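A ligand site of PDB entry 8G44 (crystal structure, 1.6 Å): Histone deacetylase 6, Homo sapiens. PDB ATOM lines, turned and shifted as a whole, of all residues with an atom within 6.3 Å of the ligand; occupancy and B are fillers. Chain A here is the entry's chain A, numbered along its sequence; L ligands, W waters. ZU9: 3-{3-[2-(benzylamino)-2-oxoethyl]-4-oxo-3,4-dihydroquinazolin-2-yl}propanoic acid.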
ATOM      1  N   GLU A  35     -16.238  -3.134 -21.051  1.00  0.00           N
ATOM      2  CA  GLU A  35     -14.988  -3.471 -20.352  1.00  0.00           C
ATOM      3  C   GLU A  35     -14.032  -4.217 -21.290  1.00  0.00           C
ATOM      4  O   GLU A  35     -13.384  -5.198 -20.918  1.00  0.00           O
ATOM      5  CB  GLU A  35     -15.364  -4.253 -19.117  1.00  0.00           C
ATOM      6  CG  GLU A  35     -14.306  -4.174 -18.086  1.00  0.00           C
ATOM      7  CD  GLU A  35     -14.918  -4.144 -16.687  1.00  0.00           C
ATOM      8  OE1 GLU A  35     -15.670  -3.199 -16.323  1.00  0.00           O
ATOM      9  OE2 GLU A  35     -14.618  -5.085 -15.946  1.00  0.00           O
ATOM     10  N   TRP A  37     -10.472  -4.559 -23.502  1.00  0.00           N
ATOM     11  CA  TRP A  37      -9.024  -4.279 -23.505  1.00  0.00           C
ATOM     12  C   TRP A  37      -8.529  -4.399 -24.947  1.00  0.00           C
ATOM     13  O   TRP A  37      -9.157  -5.074 -25.741  1.00  0.00           O
ATOM     14  CB  TRP A  37      -8.304  -5.251 -22.571  1.00  0.00           C
ATOM     15  CG  TRP A  37      -8.712  -5.125 -21.130  1.00  0.00           C
ATOM     16  CD1 TRP A  37      -9.845  -5.595 -20.544  1.00  0.00           C
ATOM     17  CD2 TRP A  37      -7.895  -4.619 -20.058  1.00  0.00           C
ATOM     18  NE1 TRP A  37      -9.870  -5.283 -19.211  1.00  0.00           N
ATOM     19  CE2 TRP A  37      -8.684  -4.676 -18.884  1.00  0.00           C
ATOM     20  CE3 TRP A  37      -6.604  -4.060 -19.989  1.00  0.00           C
ATOM     21  CZ2 TRP A  37      -8.188  -4.282 -17.647  1.00  0.00           C
ATOM     22  CZ3 TRP A  37      -6.119  -3.662 -18.769  1.00  0.00           C
ATOM     23  CH2 TRP A  37      -6.912  -3.779 -17.618  1.00  0.00           C
ATOM     24  N   CYS A  47     -12.899  -8.692 -24.491  1.00  0.00           N
ATOM     25  CA  CYS A  47     -13.484  -8.267 -23.204  1.00  0.00           C
ATOM     26  C   CYS A  47     -12.684  -8.775 -22.010  1.00  0.00           C
ATOM     27  O   CYS A  47     -11.927  -9.751 -22.059  1.00  0.00           O
ATOM     28  CB  CYS A  47     -14.957  -8.673 -23.105  1.00  0.00           C
ATOM     29  SG  CYS A  47     -15.259 -10.445 -23.102  1.00  0.00           S
ATOM     30  N   GLY A  48     -12.883  -8.047 -20.930  1.00  0.00           N
ATOM     31  CA  GLY A  48     -12.227  -8.294 -19.644  1.00  0.00           C
ATOM     32  C   GLY A  48     -12.799  -9.490 -18.896  1.00  0.00           C
ATOM     33  O   GLY A  48     -13.830 -10.022 -19.208  1.00  0.00           O
ATOM     34  N   ARG A  49     -12.052  -9.931 -17.885  1.00  0.00           N
ATOM     35  CA  ARG A  49     -12.346 -11.117 -17.071  1.00  0.00           C
ATOM     36  C   ARG A  49     -13.712 -11.054 -16.398  1.00  0.00           C
ATOM     37  O   ARG A  49     -14.273 -12.134 -16.157  1.00  0.00           O
ATOM     38  CB  ARG A  49     -11.202 -11.363 -16.110  1.00  0.00           C
ATOM     39  CG  ARG A  49     -11.102 -10.336 -14.998  1.00  0.00           C
ATOM     40  CD  ARG A  49      -9.700 -10.256 -14.465  1.00  0.00           C
ATOM     41  NE  ARG A  49      -9.492  -9.328 -13.396  1.00  0.00           N
ATOM     42  CZ  ARG A  49      -9.600  -9.539 -12.106  1.00  0.00           C
ATOM     43  NH1 ARG A  49      -9.234  -8.575 -11.278  1.00  0.00           N
ATOM     44  NH2 ARG A  49     -10.012 -10.705 -11.651  1.00  0.00           N
ATOM     45  N   TYR A  50     -14.226  -9.881 -16.081  1.00  0.00           N
ATOM     46  CA  TYR A  50     -15.528  -9.782 -15.376  1.00  0.00           C
ATOM     47  C   TYR A  50     -16.659  -9.826 -16.374  1.00  0.00           C
ATOM     48  O   TYR A  50     -17.820  -9.986 -15.927  1.00  0.00           O
ATOM     49  CB  TYR A  50     -15.571  -8.510 -14.523  1.00  0.00           C
ATOM     50  CG  TYR A  50     -14.623  -8.520 -13.359  1.00  0.00           C
ATOM     51  CD1 TYR A  50     -14.639  -9.557 -12.436  1.00  0.00           C
ATOM     52  CD2 TYR A  50     -13.696  -7.512 -13.181  1.00  0.00           C
ATOM     53  CE1 TYR A  50     -13.822  -9.553 -11.326  1.00  0.00           C
ATOM     54  CE2 TYR A  50     -12.885  -7.471 -12.064  1.00  0.00           C
ATOM     55  CZ  TYR A  50     -12.905  -8.524 -11.158  1.00  0.00           C
ATOM     56  OH  TYR A  50     -12.110  -8.486 -10.047  1.00  0.00           O
ATOM     57  N   GLY A  53     -14.209 -12.838 -20.466  1.00  0.00           N
ATOM     58  CA  GLY A  53     -12.822 -13.339 -20.358  1.00  0.00           C
ATOM     59  C   GLY A  53     -12.156 -13.538 -21.705  1.00  0.00           C
ATOM     60  O   GLY A  53     -11.241 -14.358 -21.772  1.00  0.00           O
ATOM     61  N   HIS A  54     -12.576 -12.863 -22.755  1.00  0.00           N
ATOM     62  CA  HIS A  54     -11.977 -13.150 -24.084  1.00  0.00           C
ATOM     63  C   HIS A  54     -10.549 -12.631 -24.177  1.00  0.00           C
ATOM     64  O   HIS A  54      -9.810 -13.175 -24.935  1.00  0.00           O
ATOM     65  CB  HIS A  54     -12.870 -12.744 -25.253  1.00  0.00           C
ATOM     66  CG  HIS A  54     -14.110 -13.564 -25.257  1.00  0.00           C
ATOM     67  ND1 HIS A  54     -15.407 -13.035 -25.297  1.00  0.00           N
ATOM     68  CD2 HIS A  54     -14.235 -14.916 -25.229  1.00  0.00           C
ATOM     69  CE1 HIS A  54     -16.261 -14.039 -25.234  1.00  0.00           C
ATOM     70  NE2 HIS A  54     -15.576 -15.214 -25.239  1.00  0.00           N
ATOM     71  N   MET A  55     -10.181 -11.558 -23.510  1.00  0.00           N
ATOM     72  CA  MET A  55      -8.779 -11.137 -23.625  1.00  0.00           C
ATOM     73  C   MET A  55      -7.889 -12.128 -22.864  1.00  0.00           C
ATOM     74  O   MET A  55      -6.802 -12.435 -23.364  1.00  0.00           O
ATOM     75  CB  MET A  55      -8.555  -9.714 -23.126  1.00  0.00           C
ATOM     76  CG  MET A  55      -7.148  -9.207 -23.420  1.00  0.00           C
ATOM     77  SD  MET A  55      -6.687  -9.211 -25.170  1.00  0.00           S
ATOM     78  CE  MET A  55      -7.402  -7.631 -25.629  1.00  0.00           C
ATOM     79  N   LEU A  56      -8.358 -12.713 -21.779  1.00  0.00           N
ATOM     80  CA  LEU A  56      -7.554 -13.704 -21.038  1.00  0.00           C
ATOM     81  C   LEU A  56      -7.432 -14.962 -21.923  1.00  0.00           C
ATOM     82  O   LEU A  56      -6.352 -15.564 -21.977  1.00  0.00           O
ATOM     83  CB  LEU A  56      -8.245 -13.970 -19.694  1.00  0.00           C
ATOM     84  CG  LEU A  56      -7.576 -14.992 -18.792  1.00  0.00           C
ATOM     85  CD1 LEU A  56      -6.154 -14.620 -18.449  1.00  0.00           C
ATOM     86  CD2 LEU A  56      -8.387 -15.173 -17.514  1.00  0.00           C
ATOM     87  N   VAL A  67      -1.875  -5.679 -22.205  1.00  0.00           N
ATOM     88  CA  VAL A  67      -3.207  -5.236 -22.691  1.00  0.00           C
ATOM     89  C   VAL A  67      -3.542  -3.915 -22.012  1.00  0.00           C
ATOM     90  O   VAL A  67      -3.187  -3.719 -20.869  1.00  0.00           O
ATOM     91  CB  VAL A  67      -4.275  -6.339 -22.470  1.00  0.00           C
ATOM     92  CG1 VAL A  67      -3.943  -7.553 -23.329  1.00  0.00           C
ATOM     93  CG2 VAL A  67      -4.433  -6.697 -21.013  1.00  0.00           C
ATOM     94  N   SER A  69      -6.540  -1.025 -21.041  1.00  0.00           N
ATOM     95  CA  SER A  69      -7.995  -0.925 -20.725  1.00  0.00           C
ATOM     96  C   SER A  69      -8.634   0.230 -21.486  1.00  0.00           C
ATOM     97  O   SER A  69      -8.188   1.399 -21.296  1.00  0.00           O
ATOM     98  CB  SER A  69      -8.233  -0.753 -19.269  1.00  0.00           C
ATOM     99  OG  SER A  69      -9.607  -0.424 -19.045  1.00  0.00           O
ATOM    100  N   ILE A  71     -11.386   1.373 -20.501  1.00  0.00           N
ATOM    101  CA  ILE A  71     -12.094   2.084 -19.389  1.00  0.00           C
ATOM    102  C   ILE A  71     -11.142   3.097 -18.782  1.00  0.00           C
ATOM    103  O   ILE A  71     -11.503   4.277 -18.762  1.00  0.00           O
ATOM    104  CB  ILE A  71     -12.647   1.080 -18.362  1.00  0.00           C
ATOM    105  CG1 ILE A  71     -13.736   0.218 -19.009  1.00  0.00           C
ATOM    106  CG2 ILE A  71     -13.174   1.789 -17.107  1.00  0.00           C
ATOM    107  CD1 ILE A  71     -14.421  -0.699 -18.034  1.00  0.00           C
ATOM    108  N   ASP A  72      -9.981   2.674 -18.278  1.00  0.00           N
ATOM    109  CA  ASP A  72      -9.192   3.569 -17.397  1.00  0.00           C
ATOM    110  C   ASP A  72      -7.760   3.749 -17.922  1.00  0.00           C
ATOM    111  O   ASP A  72      -6.994   4.442 -17.278  1.00  0.00           O
ATOM    112  CB  ASP A  72      -9.164   3.116 -15.930  1.00  0.00           C
ATOM    113  CG  ASP A  72      -8.410   1.835 -15.667  1.00  0.00           C
ATOM    114  OD1 ASP A  72      -7.888   1.218 -16.633  1.00  0.00           O
ATOM    115  OD2 ASP A  72      -8.291   1.467 -14.474  1.00  0.00           O
ATOM    116  N   SER A  74      -5.312   1.851 -18.004  1.00  0.00           N
ATOM    117  CA  SER A  74      -4.280   1.050 -17.324  1.00  0.00           C
ATOM    118  C   SER A  74      -3.770  -0.037 -18.274  1.00  0.00           C
ATOM    119  O   SER A  74      -4.522  -0.524 -19.167  1.00  0.00           O
ATOM    120  CB  SER A  74      -4.734   0.471 -16.025  1.00  0.00           C
ATOM    121  OG  SER A  74      -5.750  -0.515 -16.206  1.00  0.00           O
ATOM    122  N   TRP A  76      -2.056  -3.833 -18.190  1.00  0.00           N
ATOM    123  CA  TRP A  76      -1.839  -5.073 -17.409  1.00  0.00           C
ATOM    124  C   TRP A  76      -0.918  -6.008 -18.178  1.00  0.00           C
ATOM    125  O   TRP A  76      -1.147  -6.239 -19.378  1.00  0.00           O
ATOM    126  CB  TRP A  76      -3.202  -5.779 -17.129  1.00  0.00           C
ATOM    127  CG  TRP A  76      -3.156  -7.042 -16.335  1.00  0.00           C
ATOM    128  CD1 TRP A  76      -3.209  -8.334 -16.779  1.00  0.00           C
ATOM    129  CD2 TRP A  76      -2.992  -7.127 -14.900  1.00  0.00           C
ATOM    130  NE1 TRP A  76      -3.105  -9.198 -15.732  1.00  0.00           N
ATOM    131  CE2 TRP A  76      -2.978  -8.499 -14.571  1.00  0.00           C
ATOM    132  CE3 TRP A  76      -2.913  -6.170 -13.877  1.00  0.00           C
ATOM    133  CZ2 TRP A  76      -2.884  -8.924 -13.249  1.00  0.00           C
ATOM    134  CZ3 TRP A  76      -2.758  -6.615 -12.577  1.00  0.00           C
ATOM    135  CH2 TRP A  76      -2.805  -7.959 -12.289  1.00  0.00           C
ATOM    136  N   TYR A  78      -0.035  -9.870 -18.196  1.00  0.00           N
ATOM    137  CA  TYR A  78      -0.573 -11.135 -17.675  1.00  0.00           C
ATOM    138  C   TYR A  78       0.558 -11.957 -17.037  1.00  0.00           C
ATOM    139  O   TYR A  78       0.254 -12.729 -16.101  1.00  0.00           O
ATOM    140  CB  TYR A  78      -1.199 -11.944 -18.805  1.00  0.00           C
ATOM    141  CG  TYR A  78      -2.530 -11.443 -19.279  1.00  0.00           C
ATOM    142  CD1 TYR A  78      -3.650 -11.615 -18.487  1.00  0.00           C
ATOM    143  CD2 TYR A  78      -2.681 -10.854 -20.516  1.00  0.00           C
ATOM    144  CE1 TYR A  78      -4.898 -11.190 -18.929  1.00  0.00           C
ATOM    145  CE2 TYR A  78      -3.901 -10.428 -20.965  1.00  0.00           C
ATOM    146  CZ  TYR A  78      -5.019 -10.600 -20.164  1.00  0.00           C
ATOM    147  OH  TYR A  78      -6.221 -10.189 -20.687  1.00  0.00           O
ATOM    148  N   GLN A  81       1.683 -10.211 -13.800  1.00  0.00           N
ATOM    149  CA  GLN A  81       0.492 -10.120 -12.914  1.00  0.00           C
ATOM    150  C   GLN A  81       0.480  -8.769 -12.192  1.00  0.00           C
ATOM    151  O   GLN A  81       0.331  -8.667 -10.946  1.00  0.00           O
ATOM    152  CB  GLN A  81       0.439 -11.317 -11.949  1.00  0.00           C
ATOM    153  CG  GLN A  81       0.574 -12.643 -12.641  1.00  0.00           C
ATOM    154  CD  GLN A  81       0.483 -13.717 -11.580  1.00  0.00           C
ATOM    155  OE1 GLN A  81      -0.597 -14.107 -11.184  1.00  0.00           O
ATOM    156  NE2 GLN A  81       1.630 -14.125 -11.075  1.00  0.00           N
ATOM    157  N   TYR A  83       0.169  -4.126 -13.114  1.00  0.00           N
ATOM    158  CA  TYR A  83       0.051  -2.932 -13.975  1.00  0.00           C
ATOM    159  C   TYR A  83       1.463  -2.452 -14.256  1.00  0.00           C
ATOM    160  O   TYR A  83       2.360  -2.568 -13.398  1.00  0.00           O
ATOM    161  CB  TYR A  83      -0.800  -1.833 -13.349  1.00  0.00           C
ATOM    162  CG  TYR A  83      -2.209  -2.269 -13.053  1.00  0.00           C
ATOM    163  CD1 TYR A  83      -3.149  -2.296 -14.068  1.00  0.00           C
ATOM    164  CD2 TYR A  83      -2.598  -2.573 -11.756  1.00  0.00           C
ATOM    165  CE1 TYR A  83      -4.450  -2.687 -13.805  1.00  0.00           C
ATOM    166  CE2 TYR A  83      -3.890  -2.970 -11.484  1.00  0.00           C
ATOM    167  CZ  TYR A  83      -4.797  -3.048 -12.521  1.00  0.00           C
ATOM    168  OH  TYR A  83      -6.091  -3.402 -12.254  1.00  0.00           O
HETATM  169  N   ZU9 L   1      -6.505  -9.650 -16.106  1.00  0.00           N
HETATM  170  C   ZU9 L   1      -6.915  -7.458 -17.012  1.00  0.00           C
HETATM  171  O   ZU9 L   1      -9.326  -8.830 -17.665  1.00  0.00           O
HETATM  172  O3  ZU9 L   1      -6.306  -8.115 -12.358  1.00  0.00           O
HETATM  173  C10 ZU9 L   1      -6.281  -8.614 -13.469  1.00  0.00           C
HETATM  174  C9  ZU9 L   1      -6.234 -10.045 -13.700  1.00  0.00           C
HETATM  175  C8  ZU9 L   1      -6.132 -10.943 -12.637  1.00  0.00           C
HETATM  176  C7  ZU9 L   1      -6.094 -12.307 -12.896  1.00  0.00           C
HETATM  177  C6  ZU9 L   1      -6.144 -12.776 -14.189  1.00  0.00           C
HETATM  178  C5  ZU9 L   1      -6.261 -11.893 -15.257  1.00  0.00           C
HETATM  179  C4  ZU9 L   1      -6.324 -10.526 -15.013  1.00  0.00           C
HETATM  180  N1  ZU9 L   1      -6.451  -7.822 -14.615  1.00  0.00           N
HETATM  181  C3  ZU9 L   1      -6.586  -8.386 -15.885  1.00  0.00           C
HETATM  182  C1  ZU9 L   1      -7.154  -8.168 -18.331  1.00  0.00           C
HETATM  183  C2  ZU9 L   1      -8.331  -9.120 -18.394  1.00  0.00           C
HETATM  184  O1  ZU9 L   1      -8.315 -10.122 -19.061  1.00  0.00           O
HETATM  185  C11 ZU9 L   1      -6.532  -6.381 -14.408  1.00  0.00           C
HETATM  186  C12 ZU9 L   1      -7.946  -6.002 -13.984  1.00  0.00           C
HETATM  187  O2  ZU9 L   1      -8.911  -6.761 -14.260  1.00  0.00           O
HETATM  188  N2  ZU9 L   1      -8.067  -4.849 -13.313  1.00  0.00           N
HETATM  189  C13 ZU9 L   1      -9.370  -4.286 -12.951  1.00  0.00           C
HETATM  190  C14 ZU9 L   1      -9.955  -3.497 -14.101  1.00  0.00           C
HETATM  191  C19 ZU9 L   1     -11.166  -3.894 -14.689  1.00  0.00           C
HETATM  192  C18 ZU9 L   1     -11.688  -3.177 -15.761  1.00  0.00           C
HETATM  193  C17 ZU9 L   1     -11.000  -2.065 -16.254  1.00  0.00           C
HETATM  194  C16 ZU9 L   1      -9.799  -1.702 -15.711  1.00  0.00           C
HETATM  195  C15 ZU9 L   1      -9.276  -2.418 -14.630  1.00  0.00           C
HETATM  196  O   HOH W   1     -10.588  -6.652 -16.610  1.00  0.00           O
HETATM  197  O   HOH W   2      -2.780 -12.933 -12.364  1.00  0.00           O
HETATM  198  O   HOH W   3      -5.232  -9.024  -9.909  1.00  0.00           O
HETATM  199  O   HOH W   4     -10.371 -11.346 -20.245  1.00  0.00           O
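The side-chain hydroxyl (OH) of Tyr 78 lies within hydrogen-bond range of an oxygen (O1) of the ligand, 2.7 Å away. N2 of the ligand sits at hydrogen-bond distance from OH of Tyr 83, at 2.7 Å. N of Arg 49 is in hydrogen-bond range of O of the ligand. An oxygen (O2) of the ligand is in hydrogen-bond range of the guanidinium group of Arg 49 (2.8 Å). A nitrogen (N) of the ligand sits at hydrogen-bond distance from the indole nitrogen (NE1) of Trp 76 (3.5 Å).
The side-chain hydroxyl of Tyr 78 lies within hydrogen-bond range of the backbone NH of Leu 56 (3.5 Å). The guanidinium group of Arg 49 lies within hydrogen-bond range of the side-chain hydroxyl of Tyr 50, at 3.1 Å. N of Trp 76 sits at hydrogen-bond distance from O of Val 67. N of Gly 48 lies within hydrogen-bond range of O of Glu 35 (2.9 Å). OG of Ser 69 sits at hydrogen-bond distance from N of Ile 71, at 2.9 Å. O of Ser 74 sits at hydrogen-bond distance from N of Ser 69 (2.8 Å). The backbone NH of Gly 53 lies within hydrogen-bond range of the backbone carbonyl oxygen of Gly 48 (3.1 Å). The side-chain carboxylate of Asp 72 is in hydrogen-bond range of the side-chain hydroxyl of Ser 74.
Glu 35 touches the ligand. Trp 37 touches the ligand. CA of Gly 48 touches O of the ligand, 3.6 Å away. N of Leu 56 touches O1 of the ligand (3.8 Å). Ser 69 touches the ligand. Asp 72 touches the ligand (OD1 to C16, 3.6 Å). Ten residues have an atom within 4 Å of the ligand: Glu 35, Trp 37, Gly 48, Arg 49, Leu 56, Ser 69, Asp 72, Trp 76, Tyr 78 and Tyr 83. The nearest printed residue that does not touch the ligand is Ile 71 (4.1 Å).
Water W1 lies within hydrogen-bond range of an oxygen (O) of the ligand (2.7 Å) and the indole nitrogen of Trp 37 (3.0 Å).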
